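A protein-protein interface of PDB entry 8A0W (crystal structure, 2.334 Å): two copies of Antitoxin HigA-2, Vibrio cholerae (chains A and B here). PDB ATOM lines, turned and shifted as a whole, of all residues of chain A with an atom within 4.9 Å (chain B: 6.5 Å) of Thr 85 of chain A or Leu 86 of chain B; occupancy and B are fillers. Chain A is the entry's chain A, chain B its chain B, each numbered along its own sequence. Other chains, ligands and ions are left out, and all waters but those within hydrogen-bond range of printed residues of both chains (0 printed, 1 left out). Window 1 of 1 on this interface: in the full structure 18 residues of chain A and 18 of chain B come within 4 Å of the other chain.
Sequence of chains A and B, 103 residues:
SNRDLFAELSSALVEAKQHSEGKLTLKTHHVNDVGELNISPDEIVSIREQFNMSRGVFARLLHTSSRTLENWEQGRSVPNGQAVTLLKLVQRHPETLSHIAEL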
ATOM      1  N   LEU A  37       7.601 -20.227  19.954  1.00  0.00           N
ATOM      2  CA  LEU A  37       7.886 -20.500  21.357  1.00  0.00           C
ATOM      3  C   LEU A  37       6.632 -20.363  22.207  1.00  0.00           C
ATOM      4  O   LEU A  37       5.823 -19.447  22.023  1.00  0.00           O
ATOM      5  CB  LEU A  37       8.953 -19.555  21.898  1.00  0.00           C
ATOM      6  CG  LEU A  37      10.335 -19.482  21.263  1.00  0.00           C
ATOM      7  CD1 LEU A  37      11.115 -18.339  21.922  1.00  0.00           C
ATOM      8  CD2 LEU A  37      11.065 -20.806  21.395  1.00  0.00           C
ATOM      9  N   GLY A  81       4.301 -12.458  23.695  1.00  0.00           N
ATOM     10  CA  GLY A  81       5.385 -13.126  22.979  1.00  0.00           C
ATOM     11  C   GLY A  81       6.764 -12.755  23.496  1.00  0.00           C
ATOM     12  O   GLY A  81       7.640 -13.613  23.638  1.00  0.00           O
ATOM     13  N   GLN A  82       6.983 -11.477  23.781  1.00  0.00           N
ATOM     14  CA  GLN A  82       8.298 -11.074  24.266  1.00  0.00           C
ATOM     15  C   GLN A  82       8.551 -11.582  25.675  1.00  0.00           C
ATOM     16  O   GLN A  82       9.703 -11.859  26.036  1.00  0.00           O
ATOM     17  CB  GLN A  82       8.450  -9.560  24.207  1.00  0.00           C
ATOM     18  CG  GLN A  82       8.440  -9.008  22.798  1.00  0.00           C
ATOM     19  CD  GLN A  82       7.079  -9.112  22.149  1.00  0.00           C
ATOM     20  OE1 GLN A  82       6.066  -8.835  22.783  1.00  0.00           O
ATOM     21  NE2 GLN A  82       7.048  -9.502  20.864  1.00  0.00           N
ATOM     22  N   ALA A  83       7.494 -11.726  26.477  1.00  0.00           N
ATOM     23  CA  ALA A  83       7.663 -12.294  27.806  1.00  0.00           C
ATOM     24  C   ALA A  83       8.079 -13.759  27.721  1.00  0.00           C
ATOM     25  O   ALA A  83       8.925 -14.219  28.500  1.00  0.00           O
ATOM     26  CB  ALA A  83       6.375 -12.146  28.617  1.00  0.00           C
ATOM     27  N   VAL A  84       7.503 -14.504  26.776  1.00  0.00           N
ATOM     28  CA  VAL A  84       7.926 -15.886  26.561  1.00  0.00           C
ATOM     29  C   VAL A  84       9.397 -15.935  26.159  1.00  0.00           C
ATOM     30  O   VAL A  84      10.187 -16.697  26.735  1.00  0.00           O
ATOM     31  CB  VAL A  84       7.022 -16.562  25.515  1.00  0.00           C
ATOM     32  CG1 VAL A  84       7.541 -17.967  25.161  1.00  0.00           C
ATOM     33  CG2 VAL A  84       5.597 -16.670  26.056  1.00  0.00           C
ATOM     34  N   THR A  85       9.790 -15.124  25.170  1.00  0.00           N
ATOM     35  CA  THR A  85      11.193 -15.044  24.768  1.00  0.00           C
ATOM     36  C   THR A  85      12.100 -14.713  25.955  1.00  0.00           C
ATOM     37  O   THR A  85      13.120 -15.377  26.167  1.00  0.00           O
ATOM     38  CB  THR A  85      11.336 -14.000  23.662  1.00  0.00           C
ATOM     39  OG1 THR A  85      10.498 -14.362  22.554  1.00  0.00           O
ATOM     40  CG2 THR A  85      12.777 -13.893  23.180  1.00  0.00           C
ATOM     41  N   LEU A  86      11.712 -13.727  26.767  1.00  0.00           N
ATOM     42  CA  LEU A  86      12.530 -13.309  27.906  1.00  0.00           C
ATOM     43  C   LEU A  86      12.697 -14.437  28.927  1.00  0.00           C
ATOM     44  O   LEU A  86      13.815 -14.721  29.388  1.00  0.00           O
ATOM     45  CB  LEU A  86      11.899 -12.073  28.562  1.00  0.00           C
ATOM     46  CG  LEU A  86      12.729 -11.324  29.613  1.00  0.00           C
ATOM     47  CD1 LEU A  86      14.046 -10.861  29.006  1.00  0.00           C
ATOM     48  CD2 LEU A  86      11.951 -10.129  30.202  1.00  0.00           C
ATOM     49  N   LEU A  87      11.590 -15.085  29.293  1.00  0.00           N
ATOM     50  CA  LEU A  87      11.661 -16.200  30.226  1.00  0.00           C
ATOM     51  C   LEU A  87      12.591 -17.293  29.715  1.00  0.00           C
ATOM     52  O   LEU A  87      13.419 -17.813  30.467  1.00  0.00           O
ATOM     53  CB  LEU A  87      10.256 -16.760  30.488  1.00  0.00           C
ATOM     54  CG  LEU A  87       9.382 -15.869  31.373  1.00  0.00           C
ATOM     55  CD1 LEU A  87       7.908 -16.244  31.256  1.00  0.00           C
ATOM     56  CD2 LEU A  87       9.859 -15.957  32.804  1.00  0.00           C
ATOM     57  N   LYS A  88      12.473 -17.653  28.430  1.00  0.00           N
ATOM     58  CA  LYS A  88      13.302 -18.731  27.899  1.00  0.00           C
ATOM     59  C   LYS A  88      14.757 -18.300  27.780  1.00  0.00           C
ATOM     60  O   LYS A  88      15.664 -19.119  27.931  1.00  0.00           O
ATOM     61  CB  LYS A  88      12.770 -19.193  26.546  1.00  0.00           C
ATOM     62  CG  LYS A  88      11.358 -19.750  26.617  1.00  0.00           C
ATOM     63  CD  LYS A  88      11.012 -20.569  25.388  1.00  0.00           C
ATOM     64  CE  LYS A  88      10.258 -21.840  25.773  1.00  0.00           C
ATOM     65  NZ  LYS A  88      11.002 -22.673  26.780  1.00  0.00           N
ATOM     66  N   LEU A  89      14.988 -17.019  27.518  1.00  0.00           N
ATOM     67  CA  LEU A  89      16.341 -16.486  27.501  1.00  0.00           C
ATOM     68  C   LEU A  89      16.991 -16.601  28.878  1.00  0.00           C
ATOM     69  O   LEU A  89      18.132 -17.066  29.008  1.00  0.00           O
ATOM     70  CB  LEU A  89      16.276 -15.030  27.063  1.00  0.00           C
ATOM     71  CG  LEU A  89      17.539 -14.428  26.501  1.00  0.00           C
ATOM     72  CD1 LEU A  89      17.858 -15.146  25.199  1.00  0.00           C
ATOM     73  CD2 LEU A  89      17.281 -12.954  26.271  1.00  0.00           C
ATOM     74  N   LEU B  61      13.796 -12.209  13.909  1.00  0.00           N
ATOM     75  CA  LEU B  61      14.853 -12.653  14.814  1.00  0.00           C
ATOM     76  C   LEU B  61      14.498 -12.373  16.265  1.00  0.00           C
ATOM     77  O   LEU B  61      15.029 -13.027  17.168  1.00  0.00           O
ATOM     78  CB  LEU B  61      16.177 -11.979  14.435  1.00  0.00           C
ATOM     79  CG  LEU B  61      16.604 -12.236  12.983  1.00  0.00           C
ATOM     80  CD1 LEU B  61      17.905 -11.541  12.677  1.00  0.00           C
ATOM     81  CD2 LEU B  61      16.758 -13.731  12.741  1.00  0.00           C
ATOM     82  N   LEU B  62      13.593 -11.437  16.497  1.00  0.00           N
ATOM     83  CA  LEU B  62      13.097 -11.119  17.826  1.00  0.00           C
ATOM     84  C   LEU B  62      11.808 -11.864  18.165  1.00  0.00           C
ATOM     85  O   LEU B  62      11.200 -11.573  19.199  1.00  0.00           O
ATOM     86  CB  LEU B  62      12.853  -9.614  17.927  1.00  0.00           C
ATOM     87  CG  LEU B  62      13.065  -8.921  19.261  1.00  0.00           C
ATOM     88  CD1 LEU B  62      14.514  -9.030  19.701  1.00  0.00           C
ATOM     89  CD2 LEU B  62      12.623  -7.463  19.142  1.00  0.00           C
ATOM     90  N   HIS B  63      11.369 -12.792  17.310  1.00  0.00           N
ATOM     91  CA  HIS B  63      10.156 -13.576  17.545  1.00  0.00           C
ATOM     92  C   HIS B  63       8.960 -12.668  17.835  1.00  0.00           C
ATOM     93  O   HIS B  63       8.148 -12.919  18.729  1.00  0.00           O
ATOM     94  CB  HIS B  63      10.376 -14.592  18.669  1.00  0.00           C
ATOM     95  CG  HIS B  63      11.333 -15.682  18.312  1.00  0.00           C
ATOM     96  ND1 HIS B  63      11.506 -16.805  19.088  1.00  0.00           N
ATOM     97  CD2 HIS B  63      12.167 -15.825  17.255  1.00  0.00           C
ATOM     98  CE1 HIS B  63      12.407 -17.593  18.529  1.00  0.00           C
ATOM     99  NE2 HIS B  63      12.823 -17.022  17.415  1.00  0.00           N
ATOM    100  N   THR B  64       8.850 -11.607  17.035  1.00  0.00           N
ATOM    101  CA  THR B  64       7.841 -10.571  17.192  1.00  0.00           C
ATOM    102  C   THR B  64       7.083 -10.377  15.884  1.00  0.00           C
ATOM    103  O   THR B  64       7.676 -10.429  14.801  1.00  0.00           O
ATOM    104  CB  THR B  64       8.507  -9.270  17.626  1.00  0.00           C
ATOM    105  OG1 THR B  64       9.157  -9.488  18.887  1.00  0.00           O
ATOM    106  CG2 THR B  64       7.501  -8.130  17.730  1.00  0.00           C
ATOM    107  N   GLY B  81       6.109  -4.329  28.834  1.00  0.00           N
ATOM    108  CA  GLY B  81       7.307  -4.199  29.654  1.00  0.00           C
ATOM    109  C   GLY B  81       8.404  -5.163  29.252  1.00  0.00           C
ATOM    110  O   GLY B  81       9.586  -4.789  29.190  1.00  0.00           O
ATOM    111  N   GLN B  82       8.034  -6.415  28.964  1.00  0.00           N
ATOM    112  CA  GLN B  82       9.051  -7.393  28.585  1.00  0.00           C
ATOM    113  C   GLN B  82       9.613  -7.093  27.200  1.00  0.00           C
ATOM    114  O   GLN B  82      10.808  -7.306  26.957  1.00  0.00           O
ATOM    115  CB  GLN B  82       8.491  -8.821  28.657  1.00  0.00           C
ATOM    116  CG  GLN B  82       8.105  -9.255  30.061  1.00  0.00           C
ATOM    117  CD  GLN B  82       6.841  -8.556  30.543  1.00  0.00           C
ATOM    118  OE1 GLN B  82       5.917  -8.285  29.754  1.00  0.00           O
ATOM    119  NE2 GLN B  82       6.813  -8.212  31.832  1.00  0.00           N
ATOM    120  N   ALA B  83       8.785  -6.573  26.294  1.00  0.00           N
ATOM    121  CA  ALA B  83       9.310  -6.109  25.014  1.00  0.00           C
ATOM    122  C   ALA B  83      10.346  -5.016  25.213  1.00  0.00           C
ATOM    123  O   ALA B  83      11.408  -5.040  24.582  1.00  0.00           O
ATOM    124  CB  ALA B  83       8.186  -5.608  24.108  1.00  0.00           C
ATOM    125  N   VAL B  84      10.061  -4.055  26.095  1.00  0.00           N
ATOM    126  CA  VAL B  84      11.019  -2.983  26.345  1.00  0.00           C
ATOM    127  C   VAL B  84      12.337  -3.565  26.850  1.00  0.00           C
ATOM    128  O   VAL B  84      13.421  -3.189  26.384  1.00  0.00           O
ATOM    129  CB  VAL B  84      10.436  -1.956  27.331  1.00  0.00           C
ATOM    130  CG1 VAL B  84      11.462  -0.876  27.663  1.00  0.00           C
ATOM    131  CG2 VAL B  84       9.160  -1.325  26.762  1.00  0.00           C
ATOM    132  N   THR B  85      12.258  -4.494  27.811  1.00  0.00           N
ATOM    133  CA  THR B  85      13.463  -5.118  28.347  1.00  0.00           C
ATOM    134  C   THR B  85      14.250  -5.816  27.243  1.00  0.00           C
ATOM    135  O   THR B  85      15.470  -5.644  27.126  1.00  0.00           O
ATOM    136  CB  THR B  85      13.101  -6.114  29.453  1.00  0.00           C
ATOM    137  OG1 THR B  85      12.480  -5.423  30.537  1.00  0.00           O
ATOM    138  CG2 THR B  85      14.341  -6.830  29.965  1.00  0.00           C
ATOM    139  N   LEU B  86      13.551  -6.575  26.399  1.00  0.00           N
ATOM    140  CA  LEU B  86      14.199  -7.302  25.310  1.00  0.00           C
ATOM    141  C   LEU B  86      14.907  -6.357  24.348  1.00  0.00           C
ATOM    142  O   LEU B  86      16.067  -6.586  23.961  1.00  0.00           O
ATOM    143  CB  LEU B  86      13.152  -8.111  24.553  1.00  0.00           C
ATOM    144  CG  LEU B  86      13.468  -9.444  23.882  1.00  0.00           C
ATOM    145  CD1 LEU B  86      14.134 -10.410  24.840  1.00  0.00           C
ATOM    146  CD2 LEU B  86      12.162 -10.014  23.360  1.00  0.00           C
ATOM    147  N   LEU B  87      14.205  -5.300  23.918  1.00  0.00           N
ATOM    148  CA  LEU B  87      14.824  -4.324  23.030  1.00  0.00           C
ATOM    149  C   LEU B  87      16.069  -3.711  23.663  1.00  0.00           C
ATOM    150  O   LEU B  87      17.094  -3.551  22.993  1.00  0.00           O
ATOM    151  CB  LEU B  87      13.815  -3.237  22.669  1.00  0.00           C
ATOM    152  CG  LEU B  87      12.681  -3.743  21.768  1.00  0.00           C
ATOM    153  CD1 LEU B  87      11.533  -2.732  21.703  1.00  0.00           C
ATOM    154  CD2 LEU B  87      13.204  -4.034  20.382  1.00  0.00           C
ATOM    155  N   LYS B  88      16.002  -3.362  24.955  1.00  0.00           N
ATOM    156  CA  LYS B  88      17.146  -2.725  25.591  1.00  0.00           C
ATOM    157  C   LYS B  88      18.298  -3.705  25.765  1.00  0.00           C
ATOM    158  O   LYS B  88      19.458  -3.308  25.628  1.00  0.00           O
ATOM    159  CB  LYS B  88      16.733  -2.106  26.936  1.00  0.00           C
ATOM    160  CG  LYS B  88      15.789  -0.922  26.737  1.00  0.00           C
ATOM    161  CD  LYS B  88      15.756   0.014  27.908  1.00  0.00           C
ATOM    162  CE  LYS B  88      15.748   1.463  27.430  1.00  0.00           C
ATOM    163  NZ  LYS B  88      16.753   1.722  26.346  1.00  0.00           N
ATOM    164  N   LEU B  89      18.006  -4.984  26.043  1.00  0.00           N
ATOM    165  CA  LEU B  89      19.071  -5.987  26.091  1.00  0.00           C
ATOM    166  C   LEU B  89      19.783  -6.058  24.754  1.00  0.00           C
ATOM    167  O   LEU B  89      21.020  -6.050  24.689  1.00  0.00           O
ATOM    168  CB  LEU B  89      18.520  -7.372  26.451  1.00  0.00           C
ATOM    169  CG  LEU B  89      18.158  -7.637  27.908  1.00  0.00           C
ATOM    170  CD1 LEU B  89      17.544  -9.022  28.011  1.00  0.00           C
ATOM    171  CD2 LEU B  89      19.360  -7.488  28.849  1.00  0.00           C
ATOM    172  N   VAL B  90      19.004  -6.101  23.669  1.00  0.00           N
ATOM    173  CA  VAL B  90      19.589  -6.200  22.336  1.00  0.00           C
ATOM    174  C   VAL B  90      20.393  -4.952  22.022  1.00  0.00           C
ATOM    175  O   VAL B  90      21.500  -5.028  21.481  1.00  0.00           O
ATOM    176  CB  VAL B  90      18.482  -6.453  21.299  1.00  0.00           C
ATOM    177  CG1 VAL B  90      19.019  -6.284  19.889  1.00  0.00           C
ATOM    178  CG2 VAL B  90      17.951  -7.838  21.497  1.00  0.00           C
ATOM    179  N   GLN B  91      19.869  -3.785  22.396  1.00  0.00           N
ATOM    180  CA  GLN B  91      20.593  -2.541  22.179  1.00  0.00           C
ATOM    181  C   GLN B  91      21.935  -2.557  22.890  1.00  0.00           C
ATOM    182  O   GLN B  91      22.931  -2.052  22.366  1.00  0.00           O
ATOM    183  CB  GLN B  91      19.749  -1.367  22.667  1.00  0.00           C
ATOM    184  CG  GLN B  91      20.444  -0.021  22.670  1.00  0.00           C
ATOM    185  CD  GLN B  91      19.507   1.082  23.141  1.00  0.00           C
ATOM    186  OE1 GLN B  91      18.988   1.036  24.262  1.00  0.00           O
ATOM    187  NE2 GLN B  91      19.274   2.067  22.283  1.00  0.00           N
ATOM    188  N   THR B  96      22.569 -10.906  21.903  1.00  0.00           N
ATOM    189  CA  THR B  96      21.278 -11.392  22.380  1.00  0.00           C
ATOM    190  C   THR B  96      20.428 -11.902  21.226  1.00  0.00           C
ATOM    191  O   THR B  96      19.679 -12.877  21.367  1.00  0.00           O
ATOM    192  CB  THR B  96      20.550 -10.273  23.118  1.00  0.00           C
ATOM    193  OG1 THR B  96      21.386  -9.766  24.166  1.00  0.00           O
ATOM    194  CG2 THR B  96      19.251 -10.784  23.710  1.00  0.00           C
ATOM    195  N   ILE B 100      18.608 -15.621  21.086  1.00  0.00           N
ATOM    196  CA  ILE B 100      17.206 -15.933  20.843  1.00  0.00           C
ATOM    197  C   ILE B 100      17.048 -17.062  19.833  1.00  0.00           C
ATOM    198  O   ILE B 100      16.139 -17.892  19.960  1.00  0.00           O
ATOM    199  CB  ILE B 100      16.481 -14.671  20.380  1.00  0.00           C
ATOM    200  CG1 ILE B 100      16.514 -13.655  21.517  1.00  0.00           C
ATOM    201  CG2 ILE B 100      15.086 -15.030  19.918  1.00  0.00           C
ATOM    202  CD1 ILE B 100      15.600 -12.514  21.310  1.00  0.00           C
ATOM    203  N   LEU B 103      16.975 -20.686  20.937  1.00  0.00           N
ATOM    204  CA  LEU B 103      15.838 -21.133  21.741  1.00  0.00           C
ATOM    205  C   LEU B 103      14.958 -22.125  20.975  1.00  0.00           C
ATOM    206  O   LEU B 103      14.226 -21.749  20.056  1.00  0.00           O
ATOM    207  CB  LEU B 103      15.014 -19.924  22.217  1.00  0.00           C
ATOM    208  CG  LEU B 103      15.806 -18.887  23.032  1.00  0.00           C
ATOM    209  CD1 LEU B 103      14.965 -17.682  23.413  1.00  0.00           C
ATOM    210  CD2 LEU B 103      16.429 -19.509  24.271  1.00  0.00           C
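The side-chain hydroxyl (OG1) of Thr 64 of chain B lies within hydrogen-bond range of the side-chain amide nitrogen (NE2) of Gln 82 of chain A, 2.9 Å away.
The backbone carbonyl oxygen (O) of Gly 81 of chain A lies within hydrogen-bond range of the side-chain hydroxyl (OG1) of Thr 85 of chain A, 3.1 Å away. The backbone carbonyl oxygen of Leu 62 of chain B lies within hydrogen-bond range of the side-chain hydroxyl of Thr 64 of chain B (2.9 Å).
His 63 of chain B touches Leu 37 of chain A. O of Leu 103 of chain B touches CD2 of Leu 37 of chain A, at 3.6 Å. Gln 82 of chain A touches Ala 83 of chain B. Gln 82 of chain A touches Leu 86 of chain B (CB to CD2, 3.8 Å). Ala 83 of chain A touches Gln 82 of chain B (CB to CG, 3.7 Å). Thr 85 of chain A touches His 63 of chain B. Leu 86 of chain B touches Thr 85 of chain A (CD2 to CG2, 3.9 Å). Thr 85 of chain A touches Ile 100 of chain B. Lys 88 of chain A touches Leu 103 of chain B (O to CD2, 3.8 Å). Leu 89 of chain A touches Thr 96 of chain B.
Printed residues of chain B within 4 Å of Leu 37 of chain A: His 63 (3.2 Å) and Leu 103 (3.6 Å). Of the printed residues of chain B, Gln 82 of chain A touches Thr 64 (2.9 Å), Ala 83 (3.6 Å) and Leu 86 (3.8 Å). Of chain B, only His 63, Leu 86 and Ile 100 come within 4 Å of Thr 85 of chain A. Of the printed residues of chain B, Leu 86 of chain A touches Gln 82 (3.9 Å). Printed residues of chain B within 4 Å of Leu 89 of chain A: Thr 96. Leu 89 of chain B touches none of the printed residues of chain A. Printed residues of chain A within 4 Å of Leu 103 of chain B: Leu 37 and Lys 88. The nearest residue of chain B that does not touch Thr 85 of chain A is Leu 103 of chain B (4.04 Å). The nearest printed residue of chain A that does not touch Ile 100 of chain B is Leu 89 of chain A (4.2 Å).
Of the 10 printed residues of chain A, 7 touch a printed residue of chain B. Hydrophobic or aromatic side chains of chain A that line the printed part of chain B: Leu 37, Ala 83, Leu 86 and Leu 89. Printed residues of chain B that touch a printed residue of chain A: His 63, Thr 64, Gln 82, Ala 83, Leu 86, Thr 96, Ile 100 and Leu 103. Hydrophobic or aromatic side chains of chain B that line the printed part of chain A: His 63, Ala 83, Leu 86, Ile 100 and Leu 103.
Gln 82 of chain A touches Ala 83 of chain B, and with the chains exchanged Ala 83 of chain A touches Gln 82 of chain B. Gln 82 of chain A touches Leu 86 of chain B, and with the chains exchanged Leu 86 of chain A touches Gln 82 of chain B. Thr 85 of chain A touches Leu 86 of chain B, but with the chains exchanged Leu 86 of chain A does not touch Thr 85 of chain B (4.1 Å). Positions printed for both chains: 81, 82, 83, 84, 85, 86, 87, 88 and 89. Of the 12 pairs that touch across the chains among the printed residues, 4 have their exchanged pair printed and touching as well.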
